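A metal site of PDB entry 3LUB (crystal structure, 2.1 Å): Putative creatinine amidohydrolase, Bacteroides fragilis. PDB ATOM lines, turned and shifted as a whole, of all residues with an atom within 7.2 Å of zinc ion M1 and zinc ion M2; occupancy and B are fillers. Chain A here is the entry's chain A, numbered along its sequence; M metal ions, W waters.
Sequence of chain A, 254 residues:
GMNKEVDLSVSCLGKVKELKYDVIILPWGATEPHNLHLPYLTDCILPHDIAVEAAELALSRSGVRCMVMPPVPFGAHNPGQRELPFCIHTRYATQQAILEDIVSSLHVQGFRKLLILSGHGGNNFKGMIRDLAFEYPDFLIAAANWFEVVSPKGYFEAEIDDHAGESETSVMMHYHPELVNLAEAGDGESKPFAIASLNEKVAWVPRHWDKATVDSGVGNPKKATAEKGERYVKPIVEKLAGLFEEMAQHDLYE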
ATOM      1  N   GLY A  29     -19.951 -23.274  25.936  1.00  0.00           N
ATOM      2  CA  GLY A  29     -20.276 -22.826  24.640  1.00  0.00           C
ATOM      3  C   GLY A  29     -21.570 -22.038  24.567  1.00  0.00           C
ATOM      4  O   GLY A  29     -21.805 -21.127  25.356  1.00  0.00           O
ATOM      5  N   ALA A  30     -22.388 -22.402  23.596  1.00  0.00           N
ATOM      6  CA  ALA A  30     -23.582 -21.683  23.225  1.00  0.00           C
ATOM      7  C   ALA A  30     -24.363 -22.550  22.232  1.00  0.00           C
ATOM      8  O   ALA A  30     -23.778 -23.401  21.535  1.00  0.00           O
ATOM      9  CB  ALA A  30     -23.211 -20.319  22.624  1.00  0.00           C
ATOM     10  N   GLU A  32     -26.381 -21.701  19.028  1.00  0.00           N
ATOM     11  CA  GLU A  32     -26.264 -20.485  18.262  1.00  0.00           C
ATOM     12  C   GLU A  32     -26.020 -20.788  16.782  1.00  0.00           C
ATOM     13  O   GLU A  32     -25.091 -21.499  16.461  1.00  0.00           O
ATOM     14  CB  GLU A  32     -25.051 -19.666  18.771  1.00  0.00           C
ATOM     15  CG  GLU A  32     -24.822 -18.296  18.131  1.00  0.00           C
ATOM     16  CD  GLU A  32     -23.506 -17.679  18.555  1.00  0.00           C
ATOM     17  OE1 GLU A  32     -22.586 -18.449  18.829  1.00  0.00           O
ATOM     18  OE2 GLU A  32     -23.367 -16.429  18.608  1.00  0.00           O
ATOM     19  N   PRO A  33     -26.818 -20.207  15.889  1.00  0.00           N
ATOM     20  CA  PRO A  33     -26.538 -20.221  14.443  1.00  0.00           C
ATOM     21  C   PRO A  33     -25.115 -19.748  14.079  1.00  0.00           C
ATOM     22  O   PRO A  33     -24.674 -18.678  14.526  1.00  0.00           O
ATOM     23  CB  PRO A  33     -27.575 -19.250  13.886  1.00  0.00           C
ATOM     24  CG  PRO A  33     -28.672 -19.203  14.871  1.00  0.00           C
ATOM     25  CD  PRO A  33     -28.084 -19.509  16.211  1.00  0.00           C
ATOM     26  N   HIS A  34     -24.423 -20.525  13.262  1.00  0.00           N
ATOM     27  CA  HIS A  34     -23.092 -20.166  12.744  1.00  0.00           C
ATOM     28  C   HIS A  34     -23.067 -20.093  11.198  1.00  0.00           C
ATOM     29  O   HIS A  34     -22.683 -21.070  10.526  1.00  0.00           O
ATOM     30  CB  HIS A  34     -22.107 -21.229  13.204  1.00  0.00           C
ATOM     31  CG  HIS A  34     -21.633 -21.052  14.619  1.00  0.00           C
ATOM     32  ND1 HIS A  34     -22.442 -21.241  15.717  1.00  0.00           N
ATOM     33  CD2 HIS A  34     -20.429 -20.653  15.096  1.00  0.00           C
ATOM     34  CE1 HIS A  34     -21.749 -21.001  16.815  1.00  0.00           C
ATOM     35  NE2 HIS A  34     -20.520 -20.643  16.464  1.00  0.00           N
ATOM     36  N   LEU A  38     -22.260 -24.289   9.764  1.00  0.00           N
ATOM     37  CA  LEU A  38     -21.565 -24.856  10.933  1.00  0.00           C
ATOM     38  C   LEU A  38     -22.624 -25.260  11.945  1.00  0.00           C
ATOM     39  O   LEU A  38     -23.697 -24.655  12.012  1.00  0.00           O
ATOM     40  CB  LEU A  38     -20.605 -23.827  11.509  1.00  0.00           C
ATOM     41  CG  LEU A  38     -19.201 -23.687  10.915  1.00  0.00           C
ATOM     42  CD1 LEU A  38     -18.589 -22.426  11.529  1.00  0.00           C
ATOM     43  CD2 LEU A  38     -18.314 -24.913  11.177  1.00  0.00           C
ATOM     44  N   PRO A  39     -22.350 -26.297  12.745  1.00  0.00           N
ATOM     45  CA  PRO A  39     -23.323 -26.726  13.764  1.00  0.00           C
ATOM     46  C   PRO A  39     -23.732 -25.657  14.782  1.00  0.00           C
ATOM     47  O   PRO A  39     -22.917 -24.877  15.259  1.00  0.00           O
ATOM     48  CB  PRO A  39     -22.591 -27.866  14.485  1.00  0.00           C
ATOM     49  CG  PRO A  39     -21.625 -28.345  13.516  1.00  0.00           C
ATOM     50  CD  PRO A  39     -21.159 -27.161  12.752  1.00  0.00           C
ATOM     51  N   LEU A  41     -24.033 -26.220  17.690  1.00  0.00           N
ATOM     52  CA  LEU A  41     -23.225 -26.488  18.888  1.00  0.00           C
ATOM     53  C   LEU A  41     -21.719 -26.282  18.703  1.00  0.00           C
ATOM     54  O   LEU A  41     -20.911 -26.653  19.565  1.00  0.00           O
ATOM     55  CB  LEU A  41     -23.510 -27.906  19.407  1.00  0.00           C
ATOM     56  CG  LEU A  41     -24.882 -28.218  20.070  1.00  0.00           C
ATOM     57  CD1 LEU A  41     -24.822 -29.648  20.622  1.00  0.00           C
ATOM     58  CD2 LEU A  41     -25.269 -27.249  21.200  1.00  0.00           C
ATOM     59  N   THR A  42     -21.319 -25.639  17.612  1.00  0.00           N
ATOM     60  CA  THR A  42     -19.905 -25.294  17.418  1.00  0.00           C
ATOM     61  C   THR A  42     -19.147 -24.877  18.690  1.00  0.00           C
ATOM     62  O   THR A  42     -18.058 -25.369  18.969  1.00  0.00           O
ATOM     63  CB  THR A  42     -19.822 -24.205  16.309  1.00  0.00           C
ATOM     64  OG1 THR A  42     -20.239 -24.822  15.097  1.00  0.00           O
ATOM     65  CG2 THR A  42     -18.418 -23.625  16.144  1.00  0.00           C
ATOM     66  N   ASP A  43     -19.733 -23.952  19.453  1.00  0.00           N
ATOM     67  CA  ASP A  43     -19.023 -23.364  20.597  1.00  0.00           C
ATOM     68  C   ASP A  43     -18.888 -24.310  21.779  1.00  0.00           C
ATOM     69  O   ASP A  43     -18.133 -24.026  22.696  1.00  0.00           O
ATOM     70  CB  ASP A  43     -19.737 -22.092  21.072  1.00  0.00           C
ATOM     71  CG  ASP A  43     -19.687 -21.008  20.037  1.00  0.00           C
ATOM     72  OD1 ASP A  43     -18.988 -21.206  19.027  1.00  0.00           O
ATOM     73  OD2 ASP A  43     -20.348 -19.983  20.222  1.00  0.00           O
ATOM     74  N   CYS A  44     -19.649 -25.398  21.765  1.00  0.00           N
ATOM     75  CA  CYS A  44     -19.466 -26.474  22.700  1.00  0.00           C
ATOM     76  C   CYS A  44     -18.439 -27.486  22.188  1.00  0.00           C
ATOM     77  O   CYS A  44     -17.576 -27.969  22.935  1.00  0.00           O
ATOM     78  CB  CYS A  44     -20.789 -27.207  22.913  1.00  0.00           C
ATOM     79  SG  CYS A  44     -22.009 -26.278  23.808  1.00  0.00           S
ATOM     80  N   LEU A  46     -16.007 -27.405  19.838  1.00  0.00           N
ATOM     81  CA  LEU A  46     -14.604 -27.012  19.685  1.00  0.00           C
ATOM     82  C   LEU A  46     -13.803 -26.928  20.991  1.00  0.00           C
ATOM     83  O   LEU A  46     -12.725 -27.505  21.064  1.00  0.00           O
ATOM     84  CB  LEU A  46     -14.451 -25.750  18.814  1.00  0.00           C
ATOM     85  CG  LEU A  46     -14.955 -25.886  17.364  1.00  0.00           C
ATOM     86  CD1 LEU A  46     -14.631 -24.610  16.567  1.00  0.00           C
ATOM     87  CD2 LEU A  46     -14.416 -27.137  16.605  1.00  0.00           C
ATOM     88  N   ALA A  76     -24.429 -16.374  26.195  1.00  0.00           N
ATOM     89  CA  ALA A  76     -24.990 -15.035  26.317  1.00  0.00           C
ATOM     90  C   ALA A  76     -24.955 -14.411  24.935  1.00  0.00           C
ATOM     91  O   ALA A  76     -23.897 -14.347  24.318  1.00  0.00           O
ATOM     92  CB  ALA A  76     -24.128 -14.224  27.313  1.00  0.00           C
ATOM     93  N   HIS A  77     -26.110 -13.987  24.432  1.00  0.00           N
ATOM     94  CA  HIS A  77     -26.229 -13.534  23.024  1.00  0.00           C
ATOM     95  C   HIS A  77     -26.648 -12.079  22.891  1.00  0.00           C
ATOM     96  O   HIS A  77     -26.955 -11.409  23.885  1.00  0.00           O
ATOM     97  CB  HIS A  77     -27.143 -14.471  22.214  1.00  0.00           C
ATOM     98  CG  HIS A  77     -26.584 -15.849  22.108  1.00  0.00           C
ATOM     99  ND1 HIS A  77     -25.428 -16.119  21.404  1.00  0.00           N
ATOM    100  CD2 HIS A  77     -26.908 -16.996  22.757  1.00  0.00           C
ATOM    101  CE1 HIS A  77     -25.107 -17.391  21.577  1.00  0.00           C
ATOM    102  NE2 HIS A  77     -25.992 -17.937  22.398  1.00  0.00           N
ATOM    103  N   GLN A  81     -30.068 -12.022  17.679  1.00  0.00           N
ATOM    104  CA  GLN A  81     -29.729 -13.438  17.657  1.00  0.00           C
ATOM    105  C   GLN A  81     -30.839 -14.315  18.266  1.00  0.00           C
ATOM    106  O   GLN A  81     -31.052 -15.444  17.818  1.00  0.00           O
ATOM    107  CB  GLN A  81     -28.464 -13.702  18.445  1.00  0.00           C
ATOM    108  CG  GLN A  81     -27.200 -13.122  17.861  1.00  0.00           C
ATOM    109  CD  GLN A  81     -25.981 -13.755  18.497  1.00  0.00           C
ATOM    110  OE1 GLN A  81     -25.516 -13.336  19.554  1.00  0.00           O
ATOM    111  NE2 GLN A  81     -25.460 -14.793  17.841  1.00  0.00           N
ATOM    112  N   GLY A 119     -15.944 -21.303  24.317  1.00  0.00           N
ATOM    113  CA  GLY A 119     -16.015 -21.313  22.893  1.00  0.00           C
ATOM    114  C   GLY A 119     -16.809 -20.166  22.345  1.00  0.00           C
ATOM    115  O   GLY A 119     -16.861 -20.014  21.145  1.00  0.00           O
ATOM    116  N   HIS A 120     -17.397 -19.349  23.216  1.00  0.00           N
ATOM    117  CA  HIS A 120     -18.292 -18.265  22.834  1.00  0.00           C
ATOM    118  C   HIS A 120     -17.806 -16.960  23.481  1.00  0.00           C
ATOM    119  O   HIS A 120     -17.736 -16.813  24.722  1.00  0.00           O
ATOM    120  CB  HIS A 120     -19.723 -18.587  23.266  1.00  0.00           C
ATOM    121  CG  HIS A 120     -20.738 -17.522  22.954  1.00  0.00           C
ATOM    122  ND1 HIS A 120     -20.967 -17.059  21.685  1.00  0.00           N
ATOM    123  CD2 HIS A 120     -21.626 -16.878  23.759  1.00  0.00           C
ATOM    124  CE1 HIS A 120     -21.946 -16.163  21.707  1.00  0.00           C
ATOM    125  NE2 HIS A 120     -22.359 -16.027  22.952  1.00  0.00           N
ATOM    126  N   GLY A 121     -17.440 -16.010  22.626  1.00  0.00           N
ATOM    127  CA  GLY A 121     -16.888 -14.753  23.110  1.00  0.00           C
ATOM    128  C   GLY A 121     -17.903 -13.888  23.806  1.00  0.00           C
ATOM    129  O   GLY A 121     -17.524 -12.992  24.525  1.00  0.00           O
ATOM    130  N   GLY A 122     -19.188 -14.144  23.567  1.00  0.00           N
ATOM    131  CA  GLY A 122     -20.283 -13.490  24.299  1.00  0.00           C
ATOM    132  C   GLY A 122     -20.277 -13.792  25.776  1.00  0.00           C
ATOM    133  O   GLY A 122     -20.838 -13.039  26.571  1.00  0.00           O
ATOM    134  N   TRP A 146     -10.858 -20.407  23.965  1.00  0.00           N
ATOM    135  CA  TRP A 146      -9.914 -21.240  23.228  1.00  0.00           C
ATOM    136  C   TRP A 146      -9.229 -20.477  22.094  1.00  0.00           C
ATOM    137  O   TRP A 146      -8.040 -20.651  21.879  1.00  0.00           O
ATOM    138  CB  TRP A 146     -10.546 -22.599  22.729  1.00  0.00           C
ATOM    139  CG  TRP A 146     -11.476 -22.465  21.578  1.00  0.00           C
ATOM    140  CD1 TRP A 146     -12.827 -22.394  21.638  1.00  0.00           C
ATOM    141  CD2 TRP A 146     -11.131 -22.397  20.171  1.00  0.00           C
ATOM    142  NE1 TRP A 146     -13.343 -22.279  20.383  1.00  0.00           N
ATOM    143  CE2 TRP A 146     -12.330 -22.257  19.461  1.00  0.00           C
ATOM    144  CE3 TRP A 146      -9.904 -22.406  19.458  1.00  0.00           C
ATOM    145  CZ2 TRP A 146     -12.362 -22.148  18.050  1.00  0.00           C
ATOM    146  CZ3 TRP A 146      -9.938 -22.312  18.066  1.00  0.00           C
ATOM    147  CH2 TRP A 146     -11.167 -22.189  17.364  1.00  0.00           C
ATOM    148  N   PHE A 147      -9.979 -19.606  21.423  1.00  0.00           N
ATOM    149  CA  PHE A 147      -9.498 -18.865  20.247  1.00  0.00           C
ATOM    150  C   PHE A 147      -8.643 -17.629  20.535  1.00  0.00           C
ATOM    151  O   PHE A 147      -8.226 -16.931  19.597  1.00  0.00           O
ATOM    152  CB  PHE A 147     -10.692 -18.442  19.351  1.00  0.00           C
ATOM    153  CG  PHE A 147     -11.778 -17.762  20.108  1.00  0.00           C
ATOM    154  CD1 PHE A 147     -11.725 -16.392  20.345  1.00  0.00           C
ATOM    155  CD2 PHE A 147     -12.845 -18.473  20.607  1.00  0.00           C
ATOM    156  CE1 PHE A 147     -12.712 -15.769  21.049  1.00  0.00           C
ATOM    157  CE2 PHE A 147     -13.852 -17.841  21.332  1.00  0.00           C
ATOM    158  CZ  PHE A 147     -13.780 -16.507  21.559  1.00  0.00           C
ATOM    159  N   ASP A 162     -14.943 -13.096  12.866  1.00  0.00           N
ATOM    160  CA  ASP A 162     -15.432 -12.913  14.251  1.00  0.00           C
ATOM    161  C   ASP A 162     -16.378 -14.045  14.711  1.00  0.00           C
ATOM    162  O   ASP A 162     -16.441 -14.374  15.897  1.00  0.00           O
ATOM    163  CB  ASP A 162     -16.162 -11.557  14.376  1.00  0.00           C
ATOM    164  CG  ASP A 162     -15.208 -10.350  14.479  1.00  0.00           C
ATOM    165  OD1 ASP A 162     -14.010 -10.537  14.766  1.00  0.00           O
ATOM    166  OD2 ASP A 162     -15.646  -9.195  14.305  1.00  0.00           O
ATOM    167  N   HIS A 163     -17.155 -14.608  13.785  1.00  0.00           N
ATOM    168  CA  HIS A 163     -18.135 -15.633  14.133  1.00  0.00           C
ATOM    169  C   HIS A 163     -18.455 -16.493  12.938  1.00  0.00           C
ATOM    170  O   HIS A 163     -19.071 -16.012  11.976  1.00  0.00           O
ATOM    171  CB  HIS A 163     -19.434 -14.976  14.589  1.00  0.00           C
ATOM    172  CG  HIS A 163     -20.541 -15.965  14.839  1.00  0.00           C
ATOM    173  ND1 HIS A 163     -20.496 -16.888  15.848  1.00  0.00           N
ATOM    174  CD2 HIS A 163     -21.733 -16.144  14.212  1.00  0.00           C
ATOM    175  CE1 HIS A 163     -21.611 -17.606  15.831  1.00  0.00           C
ATOM    176  NE2 HIS A 163     -22.375 -17.179  14.851  1.00  0.00           N
ATOM    177  N   ALA A 164     -18.060 -17.762  13.034  1.00  0.00           N
ATOM    178  CA  ALA A 164     -18.341 -18.781  11.996  1.00  0.00           C
ATOM    179  C   ALA A 164     -17.565 -18.488  10.684  1.00  0.00           C
ATOM    180  O   ALA A 164     -17.978 -18.859   9.582  1.00  0.00           O
ATOM    181  CB  ALA A 164     -19.811 -18.882  11.740  1.00  0.00           C
ATOM    182  N   GLU A 168     -13.090 -20.615  12.806  1.00  0.00           N
ATOM    183  CA  GLU A 168     -13.981 -21.638  13.387  1.00  0.00           C
ATOM    184  C   GLU A 168     -14.254 -22.790  12.420  1.00  0.00           C
ATOM    185  O   GLU A 168     -14.311 -23.962  12.839  1.00  0.00           O
ATOM    186  CB  GLU A 168     -15.334 -21.045  13.850  1.00  0.00           C
ATOM    187  CG  GLU A 168     -15.356 -20.673  15.323  1.00  0.00           C
ATOM    188  CD  GLU A 168     -16.692 -20.175  15.833  1.00  0.00           C
ATOM    189  OE1 GLU A 168     -17.423 -19.454  15.103  1.00  0.00           O
ATOM    190  OE2 GLU A 168     -17.004 -20.479  17.013  1.00  0.00           O
ATOM    191  N   TRP A 209     -27.361  -8.421  15.468  1.00  0.00           N
ATOM    192  CA  TRP A 209     -27.279  -9.405  14.357  1.00  0.00           C
ATOM    193  C   TRP A 209     -28.283  -9.129  13.243  1.00  0.00           C
ATOM    194  O   TRP A 209     -27.987  -9.381  12.055  1.00  0.00           O
ATOM    195  CB  TRP A 209     -27.502 -10.836  14.853  1.00  0.00           C
ATOM    196  CG  TRP A 209     -26.317 -11.700  14.766  1.00  0.00           C
ATOM    197  CD1 TRP A 209     -26.138 -12.778  13.956  1.00  0.00           C
ATOM    198  CD2 TRP A 209     -25.126 -11.577  15.537  1.00  0.00           C
ATOM    199  NE1 TRP A 209     -24.908 -13.342  14.171  1.00  0.00           N
ATOM    200  CE2 TRP A 209     -24.258 -12.626  15.137  1.00  0.00           C
ATOM    201  CE3 TRP A 209     -24.688 -10.682  16.535  1.00  0.00           C
ATOM    202  CZ2 TRP A 209     -22.976 -12.803  15.694  1.00  0.00           C
ATOM    203  CZ3 TRP A 209     -23.435 -10.863  17.082  1.00  0.00           C
ATOM    204  CH2 TRP A 209     -22.588 -11.918  16.664  1.00  0.00           C
HETATM  205 ZN    ZN M   1     -18.749 -19.926  17.495  1.00  0.00          ZN
HETATM  206 ZN    ZN M   2     -20.534 -17.902  19.506  1.00  0.00          ZN
HETATM  207  O   HOH W   1     -17.703 -16.624  19.717  1.00  0.00           O
HETATM  208  O   HOH W   2     -20.917 -15.251  18.552  1.00  0.00           O
HETATM  209  O   HOH W   3     -18.821 -17.924  17.666  1.00  0.00           O
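Merely in contact with zinc ion M2: His 163 (3.8 Å).
Within 4 Å of zinc ion M2: Glu 32, Asp 43, His 120 and His 163.
Zinc ion M1 is bound by OE2 of Glu 168, 1.9 Å away.
Water W3 is bound to zinc ion M1 (2.0 Å).
Zinc ion M1 is bound by OD1 of Asp 43 (2.0 Å).
Zinc ion M1 is bound by NE2 of His 34, at 2.2 Å.
Zinc ion M1 has four donor atoms within binding distance.
Slightly farther from zinc ion M1 lies the side-chain carboxylate (OE1) of Glu 168 (2.8 Å).
Water W3 bridges ND1 of His 163 (2.7 Å) and OE1 of Glu 168 (3.3 Å).
Water W2 bridges the side-chain carboxylate of Glu 32 and a ring nitrogen (ND1) of His 163.
Zinc ion M2 is bound by OD2 of Asp 43 (2.2 Å), OE1 of Glu 32 (2.2 Å), ND1 of His 120 (2.4 Å) and water W3 (2.5 Å).
Zinc ion M2 has four donor atoms within binding distance.
Slightly farther from zinc ion M2 lies water W2 (2.8 Å).
The side-chain carboxylate (OE1) of Glu 168 sits at hydrogen-bond distance from the backbone NH (N) of Ala 164, at 2.7 Å.
ND1 of His 34 sits at hydrogen-bond distance from O of Glu 32, at 2.8 Å.
A ring nitrogen (ND1) of His 77 is in hydrogen-bond range of the side-chain carboxylate (OE2) of Glu 32.
The side-chain amide nitrogen (NE2) of Gln 81 lies within hydrogen-bond range of the side-chain carboxylate (OE2) of Glu 32.
A ring nitrogen (ND1) of His 77 lies close to a ring nitrogen (NE2) of His 120.
O of Ala 76 lies within hydrogen-bond range of NE2 of His 120, 2.7 Å away.
A ring nitrogen (NE2) of His 163 sits at hydrogen-bond distance from the backbone carbonyl oxygen of Pro 33 (2.8 Å).
OG1 of Thr 42 lies within hydrogen-bond range of O of Pro 39 (2.7 Å).
Merely in contact with zinc ion M1: Thr 42 and His 163.
Of the 26 residues printed, 5 come within 4 Å of zinc ion M1.
Along chain A the residues within 4 Å of zinc ion M1 span positions 34 to 168.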
